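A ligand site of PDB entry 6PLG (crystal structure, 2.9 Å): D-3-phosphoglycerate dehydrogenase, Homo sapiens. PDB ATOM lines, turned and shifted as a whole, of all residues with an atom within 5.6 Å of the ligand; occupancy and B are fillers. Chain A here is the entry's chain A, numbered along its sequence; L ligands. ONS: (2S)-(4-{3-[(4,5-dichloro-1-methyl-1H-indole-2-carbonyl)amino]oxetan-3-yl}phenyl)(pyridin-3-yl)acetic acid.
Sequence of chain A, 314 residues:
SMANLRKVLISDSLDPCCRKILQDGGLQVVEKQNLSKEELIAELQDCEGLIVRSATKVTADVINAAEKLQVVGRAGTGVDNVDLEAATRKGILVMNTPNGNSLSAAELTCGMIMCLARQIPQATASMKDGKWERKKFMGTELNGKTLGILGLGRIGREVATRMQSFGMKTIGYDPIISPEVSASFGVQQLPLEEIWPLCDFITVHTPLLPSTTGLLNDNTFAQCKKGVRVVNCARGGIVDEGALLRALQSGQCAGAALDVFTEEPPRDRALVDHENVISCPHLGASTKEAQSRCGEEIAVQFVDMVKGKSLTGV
The side-chain carboxylate (OD2) of Asp 174 lies within hydrogen-bond range of a nitrogen (N1) of the ligand (2.6 Å). N of Arg 154 is in hydrogen-bond range of O2 of the ligand (3.3 Å). O3 of the ligand is in salt-bridge range of NE of Arg 154.
The side-chain carboxylate of Asp 174 is in hydrogen-bond range of the backbone NH of Ile 177 (2.8 Å). The backbone NH (N) of Ile 176 lies within hydrogen-bond range of the side-chain carboxylate (OD1) of Asp 174 (2.7 Å). The side-chain carboxylate of Asp 174 sits at hydrogen-bond distance from the backbone NH of Leu 152 (3.4 Å). OG1 of Thr 206 is in hydrogen-bond range of OG1 of Thr 212 (3.4 Å). N of His 205 is in hydrogen-bond range of O of Leu 150 (2.7 Å). N of Gly 151 sits at hydrogen-bond distance from O of Tyr 173, at 3.3 Å.
Merely in contact with the ligand: Thr 206 (3.2 Å), Ile 177 (3.2 Å), His 205 (3.4 Å), Pro 175 (3.4 Å), Leu 209 (3.5 Å), Gly 153 (3.5 Å), Ile 176 (3.5 Å), Ile 155 (3.5 Å), Arg 235 (3.6 Å), Tyr 173 (3.6 Å), Pro 207 (3.7 Å), Leu 152 (3.8 Å), Ala 234 (3.9 Å) and Ser 211 (3.9 Å). Hydrophobic or aromatic side chains that line the ligand: Ile 155, Tyr 173, Pro 175, Ile 176, Ile 177, Pro 207, Leu 209 and Ala 234.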
ATOM      1  N   SER A 102      -1.991 -29.411 -10.835  1.00  0.00           N
ATOM      2  CA  SER A 102      -1.145 -28.343 -11.430  1.00  0.00           C
ATOM      3  C   SER A 102       0.080 -28.942 -12.155  1.00  0.00           C
ATOM      4  O   SER A 102       0.227 -28.741 -13.379  1.00  0.00           O
ATOM      5  CB  SER A 102      -0.713 -27.317 -10.429  1.00  0.00           C
ATOM      6  OG  SER A 102      -0.722 -27.795  -9.083  1.00  0.00           O
ATOM      7  N   LEU A 150      -0.029 -16.867 -21.249  1.00  0.00           N
ATOM      8  CA  LEU A 150      -1.298 -16.156 -20.941  1.00  0.00           C
ATOM      9  C   LEU A 150      -2.006 -16.932 -19.819  1.00  0.00           C
ATOM     10  O   LEU A 150      -2.638 -17.960 -20.128  1.00  0.00           O
ATOM     11  CB  LEU A 150      -2.158 -16.080 -22.209  1.00  0.00           C
ATOM     12  CG  LEU A 150      -1.455 -15.577 -23.467  1.00  0.00           C
ATOM     13  CD1 LEU A 150      -2.433 -15.553 -24.633  1.00  0.00           C
ATOM     14  CD2 LEU A 150      -0.802 -14.223 -23.217  1.00  0.00           C
ATOM     15  N   GLY A 151      -1.875 -16.463 -18.583  1.00  0.00           N
ATOM     16  CA  GLY A 151      -2.578 -17.053 -17.433  1.00  0.00           C
ATOM     17  C   GLY A 151      -1.591 -17.497 -16.362  1.00  0.00           C
ATOM     18  O   GLY A 151      -1.435 -18.713 -16.190  1.00  0.00           O
ATOM     19  N   LEU A 152      -1.013 -16.540 -15.641  1.00  0.00           N
ATOM     20  CA  LEU A 152       0.112 -16.750 -14.707  1.00  0.00           C
ATOM     21  C   LEU A 152      -0.447 -17.188 -13.351  1.00  0.00           C
ATOM     22  O   LEU A 152      -0.009 -16.628 -12.324  1.00  0.00           O
ATOM     23  CB  LEU A 152       0.915 -15.445 -14.609  1.00  0.00           C
ATOM     24  CG  LEU A 152       1.194 -14.723 -15.924  1.00  0.00           C
ATOM     25  CD1 LEU A 152       2.079 -13.491 -15.690  1.00  0.00           C
ATOM     26  CD2 LEU A 152       1.839 -15.674 -16.930  1.00  0.00           C
ATOM     27  N   GLY A 153      -1.331 -18.183 -13.367  1.00  0.00           N
ATOM     28  CA  GLY A 153      -1.801 -18.917 -12.169  1.00  0.00           C
ATOM     29  C   GLY A 153      -0.735 -19.857 -11.641  1.00  0.00           C
ATOM     30  O   GLY A 153       0.452 -19.469 -11.705  1.00  0.00           O
ATOM     31  N   ARG A 154      -1.119 -21.027 -11.124  1.00  0.00           N
ATOM     32  CA  ARG A 154      -0.138 -21.999 -10.570  1.00  0.00           C
ATOM     33  C   ARG A 154       0.593 -22.657 -11.756  1.00  0.00           C
ATOM     34  O   ARG A 154       1.829 -22.503 -11.855  1.00  0.00           O
ATOM     35  CB  ARG A 154      -0.812 -23.050  -9.669  1.00  0.00           C
ATOM     36  CG  ARG A 154      -2.308 -23.245  -9.887  1.00  0.00           C
ATOM     37  CD  ARG A 154      -2.671 -24.716  -9.746  1.00  0.00           C
ATOM     38  NE  ARG A 154      -3.679 -25.047  -8.743  1.00  0.00           N
ATOM     39  CZ  ARG A 154      -3.468 -25.125  -7.430  1.00  0.00           C
ATOM     40  NH1 ARG A 154      -2.280 -24.861  -6.907  1.00  0.00           N
ATOM     41  NH2 ARG A 154      -4.472 -25.472  -6.627  1.00  0.00           N
ATOM     42  N   ILE A 155      -0.167 -23.321 -12.630  1.00  0.00           N
ATOM     43  CA  ILE A 155       0.311 -24.006 -13.855  1.00  0.00           C
ATOM     44  C   ILE A 155       1.177 -23.052 -14.660  1.00  0.00           C
ATOM     45  O   ILE A 155       2.174 -23.486 -15.214  1.00  0.00           O
ATOM     46  CB  ILE A 155      -0.873 -24.497 -14.704  1.00  0.00           C
ATOM     47  CG1 ILE A 155      -1.775 -25.465 -13.947  1.00  0.00           C
ATOM     48  CG2 ILE A 155      -0.370 -25.096 -16.015  1.00  0.00           C
ATOM     49  CD1 ILE A 155      -2.942 -25.978 -14.751  1.00  0.00           C
ATOM     50  N   GLY A 156       0.754 -21.798 -14.786  1.00  0.00           N
ATOM     51  CA  GLY A 156       1.443 -20.833 -15.665  1.00  0.00           C
ATOM     52  C   GLY A 156       2.860 -20.585 -15.202  1.00  0.00           C
ATOM     53  O   GLY A 156       3.755 -20.494 -16.055  1.00  0.00           O
ATOM     54  N   TYR A 173       0.976 -12.388 -19.833  1.00  0.00           N
ATOM     55  CA  TYR A 173      -0.086 -11.427 -19.481  1.00  0.00           C
ATOM     56  C   TYR A 173      -1.077 -12.123 -18.546  1.00  0.00           C
ATOM     57  O   TYR A 173      -1.553 -13.214 -18.846  1.00  0.00           O
ATOM     58  CB  TYR A 173      -0.824 -10.954 -20.727  1.00  0.00           C
ATOM     59  CG  TYR A 173      -1.997 -10.056 -20.397  1.00  0.00           C
ATOM     60  CD1 TYR A 173      -1.809  -8.713 -20.100  1.00  0.00           C
ATOM     61  CD2 TYR A 173      -3.289 -10.574 -20.290  1.00  0.00           C
ATOM     62  CE1 TYR A 173      -2.870  -7.908 -19.754  1.00  0.00           C
ATOM     63  CE2 TYR A 173      -4.348  -9.779 -19.930  1.00  0.00           C
ATOM     64  CZ  TYR A 173      -4.144  -8.437 -19.652  1.00  0.00           C
ATOM     65  OH  TYR A 173      -5.216  -7.617 -19.328  1.00  0.00           O
ATOM     66  N   ASP A 174      -1.402 -11.458 -17.438  1.00  0.00           N
ATOM     67  CA  ASP A 174      -2.518 -11.891 -16.559  1.00  0.00           C
ATOM     68  C   ASP A 174      -3.000 -10.669 -15.782  1.00  0.00           C
ATOM     69  O   ASP A 174      -2.247 -10.027 -15.045  1.00  0.00           O
ATOM     70  CB  ASP A 174      -2.119 -13.113 -15.727  1.00  0.00           C
ATOM     71  CG  ASP A 174      -3.101 -13.411 -14.609  1.00  0.00           C
ATOM     72  OD1 ASP A 174      -3.358 -12.483 -13.822  1.00  0.00           O
ATOM     73  OD2 ASP A 174      -3.609 -14.559 -14.534  1.00  0.00           O
ATOM     74  N   PRO A 175      -4.295 -10.316 -15.914  1.00  0.00           N
ATOM     75  CA  PRO A 175      -4.841  -9.106 -15.311  1.00  0.00           C
ATOM     76  C   PRO A 175      -5.019  -9.185 -13.783  1.00  0.00           C
ATOM     77  O   PRO A 175      -5.228  -8.147 -13.190  1.00  0.00           O
ATOM     78  CB  PRO A 175      -6.200  -8.973 -15.993  1.00  0.00           C
ATOM     79  CG  PRO A 175      -6.609 -10.405 -16.301  1.00  0.00           C
ATOM     80  CD  PRO A 175      -5.301 -11.080 -16.660  1.00  0.00           C
ATOM     81  N   ILE A 176      -4.937 -10.377 -13.199  1.00  0.00           N
ATOM     82  CA  ILE A 176      -5.132 -10.603 -11.741  1.00  0.00           C
ATOM     83  C   ILE A 176      -3.779 -10.413 -11.037  1.00  0.00           C
ATOM     84  O   ILE A 176      -3.753  -9.744  -9.992  1.00  0.00           O
ATOM     85  CB  ILE A 176      -5.700 -12.000 -11.421  1.00  0.00           C
ATOM     86  CG1 ILE A 176      -7.009 -12.305 -12.152  1.00  0.00           C
ATOM     87  CG2 ILE A 176      -5.787 -12.175  -9.913  1.00  0.00           C
ATOM     88  CD1 ILE A 176      -8.227 -11.952 -11.372  1.00  0.00           C
ATOM     89  N   ILE A 177      -2.700 -11.008 -11.563  1.00  0.00           N
ATOM     90  CA  ILE A 177      -1.398 -11.045 -10.831  1.00  0.00           C
ATOM     91  C   ILE A 177      -0.581  -9.835 -11.289  1.00  0.00           C
ATOM     92  O   ILE A 177      -0.574  -9.521 -12.489  1.00  0.00           O
ATOM     93  CB  ILE A 177      -0.688 -12.383 -10.997  1.00  0.00           C
ATOM     94  CG1 ILE A 177      -0.016 -12.410 -12.352  1.00  0.00           C
ATOM     95  CG2 ILE A 177      -1.633 -13.555 -10.781  1.00  0.00           C
ATOM     96  CD1 ILE A 177       1.368 -11.801 -12.290  1.00  0.00           C
ATOM     97  N   LEU A 192      -1.405  -7.390 -23.902  1.00  0.00           N
ATOM     98  CA  LEU A 192      -1.609  -8.397 -24.974  1.00  0.00           C
ATOM     99  C   LEU A 192      -1.127  -7.853 -26.320  1.00  0.00           C
ATOM    100  O   LEU A 192      -0.347  -8.557 -26.976  1.00  0.00           O
ATOM    101  CB  LEU A 192      -3.084  -8.791 -25.045  1.00  0.00           C
ATOM    102  CG  LEU A 192      -3.566  -9.779 -23.997  1.00  0.00           C
ATOM    103  CD1 LEU A 192      -4.829 -10.490 -24.455  1.00  0.00           C
ATOM    104  CD2 LEU A 192      -2.487 -10.803 -23.698  1.00  0.00           C
ATOM    105  N   HIS A 205      -3.016 -20.676 -20.108  1.00  0.00           N
ATOM    106  CA  HIS A 205      -3.286 -21.331 -18.795  1.00  0.00           C
ATOM    107  C   HIS A 205      -4.298 -20.489 -18.004  1.00  0.00           C
ATOM    108  O   HIS A 205      -3.997 -20.055 -16.876  1.00  0.00           O
ATOM    109  CB  HIS A 205      -1.977 -21.592 -18.027  1.00  0.00           C
ATOM    110  CG  HIS A 205      -0.980 -22.347 -18.839  1.00  0.00           C
ATOM    111  ND1 HIS A 205      -1.096 -23.688 -19.066  1.00  0.00           N
ATOM    112  CD2 HIS A 205       0.087 -21.918 -19.548  1.00  0.00           C
ATOM    113  CE1 HIS A 205      -0.129 -24.054 -19.869  1.00  0.00           C
ATOM    114  NE2 HIS A 205       0.615 -22.984 -20.180  1.00  0.00           N
ATOM    115  N   THR A 206      -5.469 -20.286 -18.597  1.00  0.00           N
ATOM    116  CA  THR A 206      -6.584 -19.498 -18.039  1.00  0.00           C
ATOM    117  C   THR A 206      -7.810 -20.392 -17.894  1.00  0.00           C
ATOM    118  O   THR A 206      -7.914 -21.404 -18.587  1.00  0.00           O
ATOM    119  CB  THR A 206      -6.910 -18.326 -18.954  1.00  0.00           C
ATOM    120  OG1 THR A 206      -7.277 -18.895 -20.214  1.00  0.00           O
ATOM    121  CG2 THR A 206      -5.757 -17.373 -19.110  1.00  0.00           C
ATOM    122  N   PRO A 207      -8.759 -20.025 -17.020  1.00  0.00           N
ATOM    123  CA  PRO A 207     -10.050 -20.700 -16.965  1.00  0.00           C
ATOM    124  C   PRO A 207     -10.854 -20.271 -18.190  1.00  0.00           C
ATOM    125  O   PRO A 207     -10.513 -19.303 -18.806  1.00  0.00           O
ATOM    126  CB  PRO A 207     -10.700 -20.259 -15.641  1.00  0.00           C
ATOM    127  CG  PRO A 207      -9.832 -19.125 -15.093  1.00  0.00           C
ATOM    128  CD  PRO A 207      -8.674 -18.920 -16.053  1.00  0.00           C
ATOM    129  N   LEU A 208     -11.898 -21.035 -18.532  1.00  0.00           N
ATOM    130  CA  LEU A 208     -12.832 -20.678 -19.633  1.00  0.00           C
ATOM    131  C   LEU A 208     -13.736 -19.521 -19.152  1.00  0.00           C
ATOM    132  O   LEU A 208     -14.608 -19.790 -18.296  1.00  0.00           O
ATOM    133  CB  LEU A 208     -13.630 -21.928 -20.002  1.00  0.00           C
ATOM    134  CG  LEU A 208     -14.800 -21.701 -20.967  1.00  0.00           C
ATOM    135  CD1 LEU A 208     -14.236 -21.393 -22.340  1.00  0.00           C
ATOM    136  CD2 LEU A 208     -15.797 -22.855 -20.940  1.00  0.00           C
ATOM    137  N   LEU A 209     -13.524 -18.322 -19.673  1.00  0.00           N
ATOM    138  CA  LEU A 209     -14.376 -17.126 -19.409  1.00  0.00           C
ATOM    139  C   LEU A 209     -14.800 -16.517 -20.746  1.00  0.00           C
ATOM    140  O   LEU A 209     -14.180 -16.774 -21.764  1.00  0.00           O
ATOM    141  CB  LEU A 209     -13.670 -16.077 -18.547  1.00  0.00           C
ATOM    142  CG  LEU A 209     -13.030 -16.553 -17.245  1.00  0.00           C
ATOM    143  CD1 LEU A 209     -12.327 -15.427 -16.520  1.00  0.00           C
ATOM    144  CD2 LEU A 209     -14.077 -17.193 -16.361  1.00  0.00           C
ATOM    145  N   SER A 211     -14.342 -13.360 -21.414  1.00  0.00           N
ATOM    146  CA  SER A 211     -13.225 -12.397 -21.637  1.00  0.00           C
ATOM    147  C   SER A 211     -12.010 -13.119 -22.226  1.00  0.00           C
ATOM    148  O   SER A 211     -11.106 -12.418 -22.725  1.00  0.00           O
ATOM    149  CB  SER A 211     -12.847 -11.652 -20.371  1.00  0.00           C
ATOM    150  OG  SER A 211     -12.920 -12.482 -19.246  1.00  0.00           O
ATOM    151  N   THR A 212     -12.024 -14.466 -22.198  1.00  0.00           N
ATOM    152  CA  THR A 212     -10.878 -15.336 -22.582  1.00  0.00           C
ATOM    153  C   THR A 212     -11.245 -16.252 -23.751  1.00  0.00           C
ATOM    154  O   THR A 212     -10.337 -16.608 -24.531  1.00  0.00           O
ATOM    155  CB  THR A 212     -10.346 -16.131 -21.391  1.00  0.00           C
ATOM    156  OG1 THR A 212      -9.267 -16.789 -22.021  1.00  0.00           O
ATOM    157  CG2 THR A 212     -11.321 -17.080 -20.768  1.00  0.00           C
ATOM    158  N   LEU A 215      -9.535 -16.114 -27.276  1.00  0.00           N
ATOM    159  CA  LEU A 215      -8.385 -15.230 -26.940  1.00  0.00           C
ATOM    160  C   LEU A 215      -7.433 -15.173 -28.137  1.00  0.00           C
ATOM    161  O   LEU A 215      -6.949 -14.086 -28.478  1.00  0.00           O
ATOM    162  CB  LEU A 215      -7.664 -15.751 -25.705  1.00  0.00           C
ATOM    163  CG  LEU A 215      -6.859 -14.664 -24.989  1.00  0.00           C
ATOM    164  CD1 LEU A 215      -7.832 -13.593 -24.575  1.00  0.00           C
ATOM    165  CD2 LEU A 215      -6.088 -15.214 -23.811  1.00  0.00           C
ATOM    166  N   ALA A 234      -5.200 -26.068 -21.450  1.00  0.00           N
ATOM    167  CA  ALA A 234      -6.081 -25.480 -20.417  1.00  0.00           C
ATOM    168  C   ALA A 234      -7.542 -25.858 -20.681  1.00  0.00           C
ATOM    169  O   ALA A 234      -7.998 -26.858 -20.107  1.00  0.00           O
ATOM    170  CB  ALA A 234      -5.862 -23.992 -20.386  1.00  0.00           C
ATOM    171  N   ARG A 235      -8.241 -25.105 -21.524  1.00  0.00           N
ATOM    172  CA  ARG A 235      -9.679 -25.337 -21.835  1.00  0.00           C
ATOM    173  C   ARG A 235      -9.892 -25.171 -23.334  1.00  0.00           C
ATOM    174  O   ARG A 235      -9.229 -24.311 -23.963  1.00  0.00           O
ATOM    175  CB  ARG A 235     -10.595 -24.383 -21.054  1.00  0.00           C
ATOM    176  CG  ARG A 235     -10.563 -24.599 -19.550  1.00  0.00           C
ATOM    177  CD  ARG A 235     -11.551 -25.618 -18.955  1.00  0.00           C
ATOM    178  NE  ARG A 235     -12.711 -25.013 -18.272  1.00  0.00           N
ATOM    179  CZ  ARG A 235     -12.663 -24.313 -17.121  1.00  0.00           C
ATOM    180  NH1 ARG A 235     -11.520 -24.136 -16.481  1.00  0.00           N
ATOM    181  NH2 ARG A 235     -13.775 -23.791 -16.614  1.00  0.00           N
HETATM  182  O2  ONS L   1      -3.482 -22.220 -13.153  1.00  0.00           O
HETATM  183  C19 ONS L   1      -4.564 -22.717 -12.723  1.00  0.00           C
HETATM  184  O3  ONS L   1      -4.642 -23.760 -12.050  1.00  0.00           O
HETATM  185  C18 ONS L   1      -5.876 -22.068 -13.025  1.00  0.00           C
HETATM  186  C20 ONS L   1      -6.331 -22.661 -14.318  1.00  0.00           C
HETATM  187  C21 ONS L   1      -7.657 -23.125 -14.419  1.00  0.00           C
HETATM  188  N2  ONS L   1      -8.110 -23.686 -15.553  1.00  0.00           N
HETATM  189  C22 ONS L   1      -7.286 -23.831 -16.605  1.00  0.00           C
HETATM  190  C23 ONS L   1      -5.947 -23.397 -16.556  1.00  0.00           C
HETATM  191  C24 ONS L   1      -5.453 -22.807 -15.393  1.00  0.00           C
HETATM  192  C15 ONS L   1      -5.702 -20.596 -12.913  1.00  0.00           C
HETATM  193  C16 ONS L   1      -5.692 -19.684 -13.969  1.00  0.00           C
HETATM  194  C17 ONS L   1      -5.479 -18.325 -13.700  1.00  0.00           C
HETATM  195  C14 ONS L   1      -5.504 -20.127 -11.615  1.00  0.00           C
HETATM  196  C13 ONS L   1      -5.289 -18.779 -11.355  1.00  0.00           C
HETATM  197  C12 ONS L   1      -5.289 -17.850 -12.389  1.00  0.00           C
HETATM  198  C9  ONS L   1      -5.085 -16.363 -12.112  1.00  0.00           C
HETATM  199  C10 ONS L   1      -3.662 -15.993 -11.704  1.00  0.00           C
HETATM  200  O1  ONS L   1      -4.111 -15.587 -10.399  1.00  0.00           O
HETATM  201  C11 ONS L   1      -5.476 -15.879 -10.722  1.00  0.00           C
HETATM  202  N1  ONS L   1      -5.582 -15.541 -13.180  1.00  0.00           N
HETATM  203  C8  ONS L   1      -6.877 -15.545 -13.525  1.00  0.00           C
HETATM  204  O   ONS L   1      -7.716 -16.149 -12.870  1.00  0.00           O
HETATM  205  C6  ONS L   1      -7.265 -14.923 -14.814  1.00  0.00           C
HETATM  206  C7  ONS L   1      -6.392 -14.684 -15.866  1.00  0.00           C
HETATM  207  N   ONS L   1      -8.512 -14.547 -15.226  1.00  0.00           N
HETATM  208  C25 ONS L   1      -9.726 -14.661 -14.385  1.00  0.00           C
HETATM  209  C5  ONS L   1      -8.494 -14.060 -16.487  1.00  0.00           C
HETATM  210  C   ONS L   1      -9.465 -13.562 -17.356  1.00  0.00           C
HETATM  211  C1  ONS L   1      -9.105 -13.135 -18.633  1.00  0.00           C
HETATM  212  C4  ONS L   1      -7.168 -14.133 -16.905  1.00  0.00           C
HETATM  213  C3  ONS L   1      -6.816 -13.711 -18.177  1.00  0.00           C
HETATM  214 CL   ONS L   1      -5.140 -13.749 -18.815  1.00  0.00          CL
HETATM  215  C2  ONS L   1      -7.758 -13.229 -19.018  1.00  0.00           C
HETATM  216 CL1  ONS L   1      -7.103 -12.734 -20.606  1.00  0.00          CL
